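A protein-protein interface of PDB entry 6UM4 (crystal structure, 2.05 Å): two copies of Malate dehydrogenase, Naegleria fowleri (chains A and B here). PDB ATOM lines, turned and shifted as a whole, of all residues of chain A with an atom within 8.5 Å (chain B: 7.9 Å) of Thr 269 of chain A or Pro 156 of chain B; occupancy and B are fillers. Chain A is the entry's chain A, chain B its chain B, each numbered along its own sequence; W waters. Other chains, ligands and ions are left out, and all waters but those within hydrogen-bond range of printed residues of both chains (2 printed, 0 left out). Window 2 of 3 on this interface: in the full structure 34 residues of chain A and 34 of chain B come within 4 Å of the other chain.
The side-chain amino group of Lys 341 of chain A sits at hydrogen-bond distance from the backbone carbonyl oxygen of Gly 153 of chain B (2.7 Å).
Hydrophobic or aromatic side chains of chain B that line the printed part of chain A: Phe 155 and Pro 156. Of the 16 printed residues of chain A, 4 touch a printed residue of chain B. Hydrophobic or aromatic side chains of chain A that line the printed part of chain B: Ile 268.
Of the printed residues of chain B, Ile 268 of chain A touches Ala 154. Of chain B, only Pro 156 (3.5 Å) comes within 4 Å of Thr 269 of chain A. Of the printed residues of chain B, Asp 337 of chain A touches Gly 153 (3.5 Å) and Phe 155 (3.2 Å). Of the printed residues of chain A, Gly 153 of chain B touches Asp 337 and Lys 341. Printed residues of chain A within 4 Å of Ala 154 of chain B: Ile 268. Of the printed residues of chain A, Phe 155 of chain B touches Asp 337 and Lys 341. Of the printed residues of chain A, Pro 156 of chain B touches Thr 269. The nearest residue of chain B that does not touch Thr 269 of chain A is Leu 157 of chain B (6.3 Å). The nearest residue of chain A that does not touch Pro 156 of chain B is Ile 268 of chain A (4.4 Å).
No position is printed for both chains.
OD2 of Asp 337 of chain A is in salt-bridge range of NZ of Lys 341 of chain A, at 2.9 Å.
Among the printed residues, merely in contact across the chains: Asp 337 of chain A with Phe 155 of chain B (3.2 Å), Thr 269 of chain A with Pro 156 of chain B (3.5 Å), Asp 337 of chain A with Gly 153 of chain B (3.5 Å), Ile 268 of chain A with Ala 154 of chain B (3.5 Å) and Lys 341 of chain A with Phe 155 of chain B (3.5 Å).
Water W2 lies within hydrogen-bond range of the backbone carbonyl oxygen (O) of Pro 156 of chain B (2.9 Å), the backbone NH (N) of Ile 268 of chain A (3.0 Å) and the backbone NH (N) of Thr 269 of chain A (3.1 Å). Water W1 bridges N of Ile 268 of chain A (3.0 Å) and O of Phe 155 of chain B (3.4 Å).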
ATOM      1  N   LEU A 257      -3.857  23.027   5.607  1.00  0.00           N
ATOM      2  CA  LEU A 257      -4.630  22.608   4.446  1.00  0.00           C
ATOM      3  C   LEU A 257      -5.051  23.806   3.616  1.00  0.00           C
ATOM      4  O   LEU A 257      -5.065  23.739   2.384  1.00  0.00           O
ATOM      5  CB  LEU A 257      -5.860  21.802   4.869  1.00  0.00           C
ATOM      6  CG  LEU A 257      -5.669  20.484   5.606  1.00  0.00           C
ATOM      7  CD1 LEU A 257      -7.020  19.903   5.915  1.00  0.00           C
ATOM      8  CD2 LEU A 257      -4.877  19.514   4.753  1.00  0.00           C
ATOM      9  N   ALA A 261      -4.031  24.608  -0.357  1.00  0.00           N
ATOM     10  CA  ALA A 261      -5.075  24.795  -1.356  1.00  0.00           C
ATOM     11  C   ALA A 261      -4.982  26.162  -2.023  1.00  0.00           C
ATOM     12  O   ALA A 261      -5.186  26.284  -3.237  1.00  0.00           O
ATOM     13  CB  ALA A 261      -6.444  24.600  -0.712  1.00  0.00           C
ATOM     14  N   CYS A 266      -5.897  23.925  -5.591  1.00  0.00           N
ATOM     15  CA  CYS A 266      -6.638  22.671  -5.633  1.00  0.00           C
ATOM     16  C   CYS A 266      -7.820  22.739  -4.675  1.00  0.00           C
ATOM     17  O   CYS A 266      -8.025  23.737  -3.979  1.00  0.00           O
ATOM     18  CB  CYS A 266      -5.727  21.488  -5.298  1.00  0.00           C
ATOM     19  SG  CYS A 266      -5.003  21.491  -3.617  1.00  0.00           S
ATOM     20  N   ASN A 267      -8.638  21.687  -4.688  1.00  0.00           N
ATOM     21  CA  ASN A 267      -9.694  21.564  -3.696  1.00  0.00           C
ATOM     22  C   ASN A 267      -9.125  20.974  -2.414  1.00  0.00           C
ATOM     23  O   ASN A 267      -8.085  20.307  -2.416  1.00  0.00           O
ATOM     24  CB  ASN A 267     -10.835  20.689  -4.212  1.00  0.00           C
ATOM     25  N   ILE A 268      -9.804  21.257  -1.301  1.00  0.00           N
ATOM     26  CA  ILE A 268      -9.398  20.691  -0.019  1.00  0.00           C
ATOM     27  C   ILE A 268      -9.377  19.173  -0.093  1.00  0.00           C
ATOM     28  O   ILE A 268      -8.501  18.518   0.486  1.00  0.00           O
ATOM     29  CB  ILE A 268     -10.326  21.187   1.104  1.00  0.00           C
ATOM     30  CG1 ILE A 268     -10.083  22.671   1.350  1.00  0.00           C
ATOM     31  CG2 ILE A 268     -10.085  20.383   2.388  1.00  0.00           C
ATOM     32  CD1 ILE A 268      -8.708  22.978   1.939  1.00  0.00           C
ATOM     33  N   THR A 269     -10.345  18.584  -0.793  1.00  0.00           N
ATOM     34  CA  THR A 269     -10.391  17.129  -0.864  1.00  0.00           C
ATOM     35  C   THR A 269      -9.273  16.529  -1.707  1.00  0.00           C
ATOM     36  O   THR A 269      -9.077  15.311  -1.645  1.00  0.00           O
ATOM     37  CB  THR A 269     -11.738  16.664  -1.407  1.00  0.00           C
ATOM     38  OG1 THR A 269     -11.997  17.306  -2.662  1.00  0.00           O
ATOM     39  CG2 THR A 269     -12.848  16.991  -0.419  1.00  0.00           C
ATOM     40  N   ASP A 270      -8.567  17.333  -2.508  1.00  0.00           N
ATOM     41  CA  ASP A 270      -7.414  16.836  -3.261  1.00  0.00           C
ATOM     42  C   ASP A 270      -6.189  16.561  -2.382  1.00  0.00           C
ATOM     43  O   ASP A 270      -5.284  15.833  -2.811  1.00  0.00           O
ATOM     44  CB  ASP A 270      -7.040  17.840  -4.355  1.00  0.00           C
ATOM     45  CG  ASP A 270      -8.152  18.040  -5.384  1.00  0.00           C
ATOM     46  OD1 ASP A 270      -8.886  17.074  -5.682  1.00  0.00           O
ATOM     47  OD2 ASP A 270      -8.283  19.168  -5.902  1.00  0.00           O
ATOM     48  N   ILE A 271      -6.140  17.127  -1.175  1.00  0.00           N
ATOM     49  CA  ILE A 271      -4.979  17.043  -0.291  1.00  0.00           C
ATOM     50  C   ILE A 271      -5.107  15.836   0.628  1.00  0.00           C
ATOM     51  O   ILE A 271      -6.144  15.641   1.274  1.00  0.00           O
ATOM     52  CB  ILE A 271      -4.841  18.338   0.525  1.00  0.00           C
ATOM     53  CG1 ILE A 271      -4.902  19.540  -0.402  1.00  0.00           C
ATOM     54  CG2 ILE A 271      -3.555  18.358   1.321  1.00  0.00           C
ATOM     55  CD1 ILE A 271      -4.940  20.865   0.340  1.00  0.00           C
ATOM     56  N   SER A 272      -4.028  15.060   0.743  1.00  0.00           N
ATOM     57  CA  SER A 272      -3.994  13.887   1.609  1.00  0.00           C
ATOM     58  C   SER A 272      -2.693  13.879   2.384  1.00  0.00           C
ATOM     59  O   SER A 272      -1.707  14.477   1.960  1.00  0.00           O
ATOM     60  CB  SER A 272      -4.098  12.563   0.830  1.00  0.00           C
ATOM     61  OG  SER A 272      -5.421  12.319   0.375  1.00  0.00           O
ATOM     62  N   ARG A 273      -2.716  13.228   3.548  1.00  0.00           N
ATOM     63  CA  ARG A 273      -1.513  12.924   4.316  1.00  0.00           C
ATOM     64  C   ARG A 273      -0.762  14.191   4.739  1.00  0.00           C
ATOM     65  O   ARG A 273       0.412  14.402   4.403  1.00  0.00           O
ATOM     66  CB  ARG A 273      -0.610  11.992   3.516  1.00  0.00           C
ATOM     67  CG  ARG A 273      -1.277  10.687   3.159  1.00  0.00           C
ATOM     68  CD  ARG A 273      -0.596  10.058   1.962  1.00  0.00           C
ATOM     69  NE  ARG A 273       0.805   9.771   2.248  1.00  0.00           N
ATOM     70  CZ  ARG A 273       1.242   8.579   2.645  1.00  0.00           C
ATOM     71  NH1 ARG A 273       0.374   7.588   2.810  1.00  0.00           N
ATOM     72  NH2 ARG A 273       2.535   8.376   2.887  1.00  0.00           N
ATOM     73  N   THR A 292       0.083  14.501  -0.460  1.00  0.00           N
ATOM     74  CA  THR A 292      -0.193  14.303  -1.876  1.00  0.00           C
ATOM     75  C   THR A 292      -1.349  15.195  -2.309  1.00  0.00           C
ATOM     76  O   THR A 292      -2.175  15.626  -1.502  1.00  0.00           O
ATOM     77  CB  THR A 292      -0.509  12.838  -2.211  1.00  0.00           C
ATOM     78  OG1 THR A 292      -1.688  12.429  -1.509  1.00  0.00           O
ATOM     79  CG2 THR A 292       0.650  11.935  -1.843  1.00  0.00           C
ATOM     80  N   ILE A 293      -1.380  15.482  -3.602  1.00  0.00           N
ATOM     81  CA  ILE A 293      -2.405  16.308  -4.212  1.00  0.00           C
ATOM     82  C   ILE A 293      -2.930  15.531  -5.405  1.00  0.00           C
ATOM     83  O   ILE A 293      -2.150  15.164  -6.291  1.00  0.00           O
ATOM     84  CB  ILE A 293      -1.855  17.675  -4.645  1.00  0.00           C
ATOM     85  CG1 ILE A 293      -1.281  18.412  -3.441  1.00  0.00           C
ATOM     86  CG2 ILE A 293      -2.939  18.503  -5.368  1.00  0.00           C
ATOM     87  CD1 ILE A 293      -0.482  19.637  -3.823  1.00  0.00           C
ATOM     88  N   LYS A 294      -4.234  15.256  -5.416  1.00  0.00           N
ATOM     89  CA  LYS A 294      -4.818  14.473  -6.501  1.00  0.00           C
ATOM     90  C   LYS A 294      -4.470  15.078  -7.861  1.00  0.00           C
ATOM     91  O   LYS A 294      -4.670  16.271  -8.094  1.00  0.00           O
ATOM     92  CB  LYS A 294      -6.335  14.386  -6.332  1.00  0.00           C
ATOM     93  N   ASP A 337     -14.835  25.940  14.790  1.00  0.00           N
ATOM     94  CA  ASP A 337     -14.926  24.981  13.691  1.00  0.00           C
ATOM     95  C   ASP A 337     -13.941  23.820  13.865  1.00  0.00           C
ATOM     96  O   ASP A 337     -14.284  22.660  13.619  1.00  0.00           O
ATOM     97  CB  ASP A 337     -14.670  25.681  12.360  1.00  0.00           C
ATOM     98  CG  ASP A 337     -14.690  24.717  11.201  1.00  0.00           C
ATOM     99  OD1 ASP A 337     -15.802  24.381  10.727  1.00  0.00           O
ATOM    100  OD2 ASP A 337     -13.593  24.294  10.766  1.00  0.00           O
ATOM    101  N   LYS A 341     -14.748  19.848  14.342  1.00  0.00           N
ATOM    102  CA  LYS A 341     -14.133  18.803  13.522  1.00  0.00           C
ATOM    103  C   LYS A 341     -13.349  17.806  14.384  1.00  0.00           C
ATOM    104  O   LYS A 341     -13.404  16.588  14.153  1.00  0.00           O
ATOM    105  CB  LYS A 341     -13.230  19.416  12.446  1.00  0.00           C
ATOM    106  CG  LYS A 341     -13.973  20.053  11.235  1.00  0.00           C
ATOM    107  CD  LYS A 341     -12.968  20.673  10.281  1.00  0.00           C
ATOM    108  CE  LYS A 341     -13.569  21.019   8.919  1.00  0.00           C
ATOM    109  NZ  LYS A 341     -14.404  22.261   8.931  1.00  0.00           N
ATOM    110  N   GLU A 352      -9.069  10.310   6.581  1.00  0.00           N
ATOM    111  CA  GLU A 352      -7.857  11.063   6.303  1.00  0.00           C
ATOM    112  C   GLU A 352      -7.036  11.224   7.571  1.00  0.00           C
ATOM    113  O   GLU A 352      -7.560  11.163   8.683  1.00  0.00           O
ATOM    114  CB  GLU A 352      -8.196  12.438   5.729  1.00  0.00           C
ATOM    115  CG  GLU A 352      -8.913  12.361   4.392  1.00  0.00           C
ATOM    116  CD  GLU A 352      -7.969  12.039   3.247  1.00  0.00           C
ATOM    117  OE1 GLU A 352      -6.744  12.270   3.392  1.00  0.00           O
ATOM    118  OE2 GLU A 352      -8.451  11.517   2.219  1.00  0.00           O
ATOM    119  N   LEU B  94     -21.656  14.801  -6.403  1.00  0.00           N
ATOM    120  CA  LEU B  94     -21.871  16.203  -6.070  1.00  0.00           C
ATOM    121  C   LEU B  94     -22.646  16.906  -7.176  1.00  0.00           C
ATOM    122  O   LEU B  94     -22.384  16.706  -8.363  1.00  0.00           O
ATOM    123  CB  LEU B  94     -20.541  16.922  -5.861  1.00  0.00           C
ATOM    124  CG  LEU B  94     -19.730  16.699  -4.586  1.00  0.00           C
ATOM    125  CD1 LEU B  94     -18.523  17.649  -4.571  1.00  0.00           C
ATOM    126  CD2 LEU B  94     -20.561  16.856  -3.326  1.00  0.00           C
ATOM    127  N   ALA B 118     -20.937  27.125   4.541  1.00  0.00           N
ATOM    128  CA  ALA B 118     -19.783  26.406   4.015  1.00  0.00           C
ATOM    129  C   ALA B 118     -19.762  24.953   4.489  1.00  0.00           C
ATOM    130  O   ALA B 118     -19.184  24.089   3.814  1.00  0.00           O
ATOM    131  CB  ALA B 118     -18.501  27.135   4.412  1.00  0.00           C
ATOM    132  N   ASN B 119     -20.369  24.658   5.651  1.00  0.00           N
ATOM    133  CA  ASN B 119     -20.347  23.287   6.155  1.00  0.00           C
ATOM    134  C   ASN B 119     -21.363  22.392   5.455  1.00  0.00           C
ATOM    135  O   ASN B 119     -21.445  21.204   5.779  1.00  0.00           O
ATOM    136  CB  ASN B 119     -20.544  23.239   7.691  1.00  0.00           C
ATOM    137  CG  ASN B 119     -21.970  23.602   8.147  1.00  0.00           C
ATOM    138  OD1 ASN B 119     -22.786  24.112   7.370  1.00  0.00           O
ATOM    139  ND2 ASN B 119     -22.272  23.317   9.421  1.00  0.00           N
ATOM    140  N   GLY B 120     -22.153  22.932   4.527  1.00  0.00           N
ATOM    141  CA  GLY B 120     -23.155  22.155   3.835  1.00  0.00           C
ATOM    142  C   GLY B 120     -24.491  22.061   4.553  1.00  0.00           C
ATOM    143  O   GLY B 120     -25.391  21.364   4.068  1.00  0.00           O
ATOM    144  N   GLU B 125     -25.417  18.332   2.218  1.00  0.00           N
ATOM    145  CA  GLU B 125     -24.038  17.864   2.314  1.00  0.00           C
ATOM    146  C   GLU B 125     -23.411  17.541   0.964  1.00  0.00           C
ATOM    147  O   GLU B 125     -22.193  17.357   0.906  1.00  0.00           O
ATOM    148  CB  GLU B 125     -23.988  16.633   3.204  1.00  0.00           C
ATOM    149  CG  GLU B 125     -24.701  15.442   2.598  1.00  0.00           C
ATOM    150  CD  GLU B 125     -24.757  14.263   3.541  1.00  0.00           C
ATOM    151  OE1 GLU B 125     -23.765  14.043   4.270  1.00  0.00           O
ATOM    152  OE2 GLU B 125     -25.797  13.567   3.564  1.00  0.00           O
ATOM    153  N   GLN B 127     -23.937  19.562  -1.851  1.00  0.00           N
ATOM    154  CA  GLN B 127     -24.152  20.755  -2.676  1.00  0.00           C
ATOM    155  C   GLN B 127     -23.004  21.741  -2.526  1.00  0.00           C
ATOM    156  O   GLN B 127     -22.989  22.538  -1.571  1.00  0.00           O
ATOM    157  CB  GLN B 127     -25.468  21.433  -2.306  1.00  0.00           C
ATOM    158  CG  GLN B 127     -25.728  22.714  -3.069  1.00  0.00           C
ATOM    159  CD  GLN B 127     -25.734  22.495  -4.556  1.00  0.00           C
ATOM    160  OE1 GLN B 127     -26.690  21.948  -5.109  1.00  0.00           O
ATOM    161  NE2 GLN B 127     -24.643  22.876  -5.213  1.00  0.00           N
ATOM    162  N   PRO B 128     -22.033  21.735  -3.441  1.00  0.00           N
ATOM    163  CA  PRO B 128     -20.939  22.712  -3.374  1.00  0.00           C
ATOM    164  C   PRO B 128     -21.449  24.136  -3.536  1.00  0.00           C
ATOM    165  O   PRO B 128     -22.423  24.402  -4.252  1.00  0.00           O
ATOM    166  CB  PRO B 128     -20.036  22.317  -4.549  1.00  0.00           C
ATOM    167  CG  PRO B 128     -20.399  20.877  -4.851  1.00  0.00           C
ATOM    168  CD  PRO B 128     -21.870  20.774  -4.542  1.00  0.00           C
ATOM    169  N   VAL B 129     -20.783  25.066  -2.854  1.00  0.00           N
ATOM    170  CA  VAL B 129     -21.246  26.449  -2.838  1.00  0.00           C
ATOM    171  C   VAL B 129     -20.098  27.395  -3.149  1.00  0.00           C
ATOM    172  O   VAL B 129     -18.928  27.121  -2.846  1.00  0.00           O
ATOM    173  CB  VAL B 129     -21.899  26.838  -1.493  1.00  0.00           C
ATOM    174  CG1 VAL B 129     -23.140  25.996  -1.253  1.00  0.00           C
ATOM    175  CG2 VAL B 129     -20.897  26.667  -0.354  1.00  0.00           C
ATOM    176  N   GLY B 153     -11.469  27.043   7.723  1.00  0.00           N
ATOM    177  CA  GLY B 153     -12.383  25.941   7.970  1.00  0.00           C
ATOM    178  C   GLY B 153     -12.145  24.716   7.114  1.00  0.00           C
ATOM    179  O   GLY B 153     -12.723  23.663   7.383  1.00  0.00           O
ATOM    180  N   ALA B 154     -11.330  24.836   6.069  1.00  0.00           N
ATOM    181  CA  ALA B 154     -10.970  23.710   5.209  1.00  0.00           C
ATOM    182  C   ALA B 154     -12.212  22.969   4.722  1.00  0.00           C
ATOM    183  O   ALA B 154     -12.277  21.740   4.739  1.00  0.00           O
ATOM    184  CB  ALA B 154     -10.009  22.757   5.931  1.00  0.00           C
ATOM    185  N   PHE B 155     -13.208  23.728   4.274  1.00  0.00           N
ATOM    186  CA  PHE B 155     -14.494  23.130   3.927  1.00  0.00           C
ATOM    187  C   PHE B 155     -14.456  22.527   2.530  1.00  0.00           C
ATOM    188  O   PHE B 155     -14.248  23.261   1.559  1.00  0.00           O
ATOM    189  CB  PHE B 155     -15.613  24.158   3.980  1.00  0.00           C
ATOM    190  CG  PHE B 155     -15.921  24.635   5.346  1.00  0.00           C
ATOM    191  CD1 PHE B 155     -16.580  23.809   6.245  1.00  0.00           C
ATOM    192  CD2 PHE B 155     -15.573  25.918   5.732  1.00  0.00           C
ATOM    193  CE1 PHE B 155     -16.895  24.257   7.494  1.00  0.00           C
ATOM    194  CE2 PHE B 155     -15.886  26.371   6.994  1.00  0.00           C
ATOM    195  CZ  PHE B 155     -16.546  25.535   7.873  1.00  0.00           C
ATOM    196  N   PRO B 156     -14.704  21.224   2.377  1.00  0.00           N
ATOM    197  CA  PRO B 156     -14.706  20.630   1.030  1.00  0.00           C
ATOM    198  C   PRO B 156     -15.755  21.192   0.087  1.00  0.00           C
ATOM    199  O   PRO B 156     -15.529  21.189  -1.130  1.00  0.00           O
ATOM    200  CB  PRO B 156     -14.938  19.140   1.303  1.00  0.00           C
ATOM    201  CG  PRO B 156     -15.411  19.048   2.708  1.00  0.00           C
ATOM    202  CD  PRO B 156     -14.878  20.225   3.440  1.00  0.00           C
ATOM    203  N   LEU B 157     -16.894  21.669   0.593  1.00  0.00           N
ATOM    204  CA  LEU B 157     -17.969  22.131  -0.276  1.00  0.00           C
ATOM    205  C   LEU B 157     -17.787  23.566  -0.762  1.00  0.00           C
ATOM    206  O   LEU B 157     -18.485  23.977  -1.693  1.00  0.00           O
ATOM    207  CB  LEU B 157     -19.313  21.986   0.445  1.00  0.00           C
ATOM    208  CG  LEU B 157     -19.798  20.551   0.649  1.00  0.00           C
ATOM    209  CD1 LEU B 157     -21.028  20.531   1.552  1.00  0.00           C
ATOM    210  CD2 LEU B 157     -20.112  19.888  -0.692  1.00  0.00           C
ATOM    211  N   LEU B 158     -16.886  24.329  -0.152  1.00  0.00           N
ATOM    212  CA  LEU B 158     -16.693  25.748  -0.450  1.00  0.00           C
ATOM    213  C   LEU B 158     -15.754  25.876  -1.646  1.00  0.00           C
ATOM    214  O   LEU B 158     -14.526  25.809  -1.509  1.00  0.00           O
ATOM    215  CB  LEU B 158     -16.143  26.469   0.775  1.00  0.00           C
ATOM    216  CG  LEU B 158     -16.084  27.994   0.759  1.00  0.00           C
ATOM    217  CD1 LEU B 158     -17.412  28.591   0.285  1.00  0.00           C
ATOM    218  CD2 LEU B 158     -15.758  28.486   2.152  1.00  0.00           C
ATOM    219  N   GLU B 159     -16.328  26.081  -2.829  1.00  0.00           N
ATOM    220  CA  GLU B 159     -15.496  26.123  -4.024  1.00  0.00           C
ATOM    221  C   GLU B 159     -14.866  27.489  -4.244  1.00  0.00           C
ATOM    222  O   GLU B 159     -13.794  27.571  -4.851  1.00  0.00           O
ATOM    223  CB  GLU B 159     -16.308  25.707  -5.251  1.00  0.00           C
ATOM    224  CG  GLU B 159     -16.720  24.250  -5.210  1.00  0.00           C
ATOM    225  CD  GLU B 159     -16.996  23.669  -6.583  1.00  0.00           C
ATOM    226  OE1 GLU B 159     -16.975  24.434  -7.573  1.00  0.00           O
ATOM    227  OE2 GLU B 159     -17.226  22.440  -6.666  1.00  0.00           O
ATOM    228  N   GLU B 160     -15.481  28.565  -3.752  1.00  0.00           N
ATOM    229  CA  GLU B 160     -14.894  29.873  -3.998  1.00  0.00           C
ATOM    230  C   GLU B 160     -15.396  30.884  -2.977  1.00  0.00           C
ATOM    231  O   GLU B 160     -16.559  30.843  -2.565  1.00  0.00           O
ATOM    232  CB  GLU B 160     -15.214  30.362  -5.416  1.00  0.00           C
ATOM    233  CG  GLU B 160     -14.474  31.631  -5.808  1.00  0.00           C
ATOM    234  CD  GLU B 160     -15.052  32.315  -7.052  1.00  0.00           C
ATOM    235  OE1 GLU B 160     -15.927  31.732  -7.735  1.00  0.00           O
ATOM    236  OE2 GLU B 160     -14.630  33.454  -7.336  1.00  0.00           O
HETATM  237  O   HOH W   1     -12.183  23.123  -1.186  1.00  0.00           O
HETATM  238  O   HOH W   2     -12.720  20.443  -1.612  1.00  0.00           O
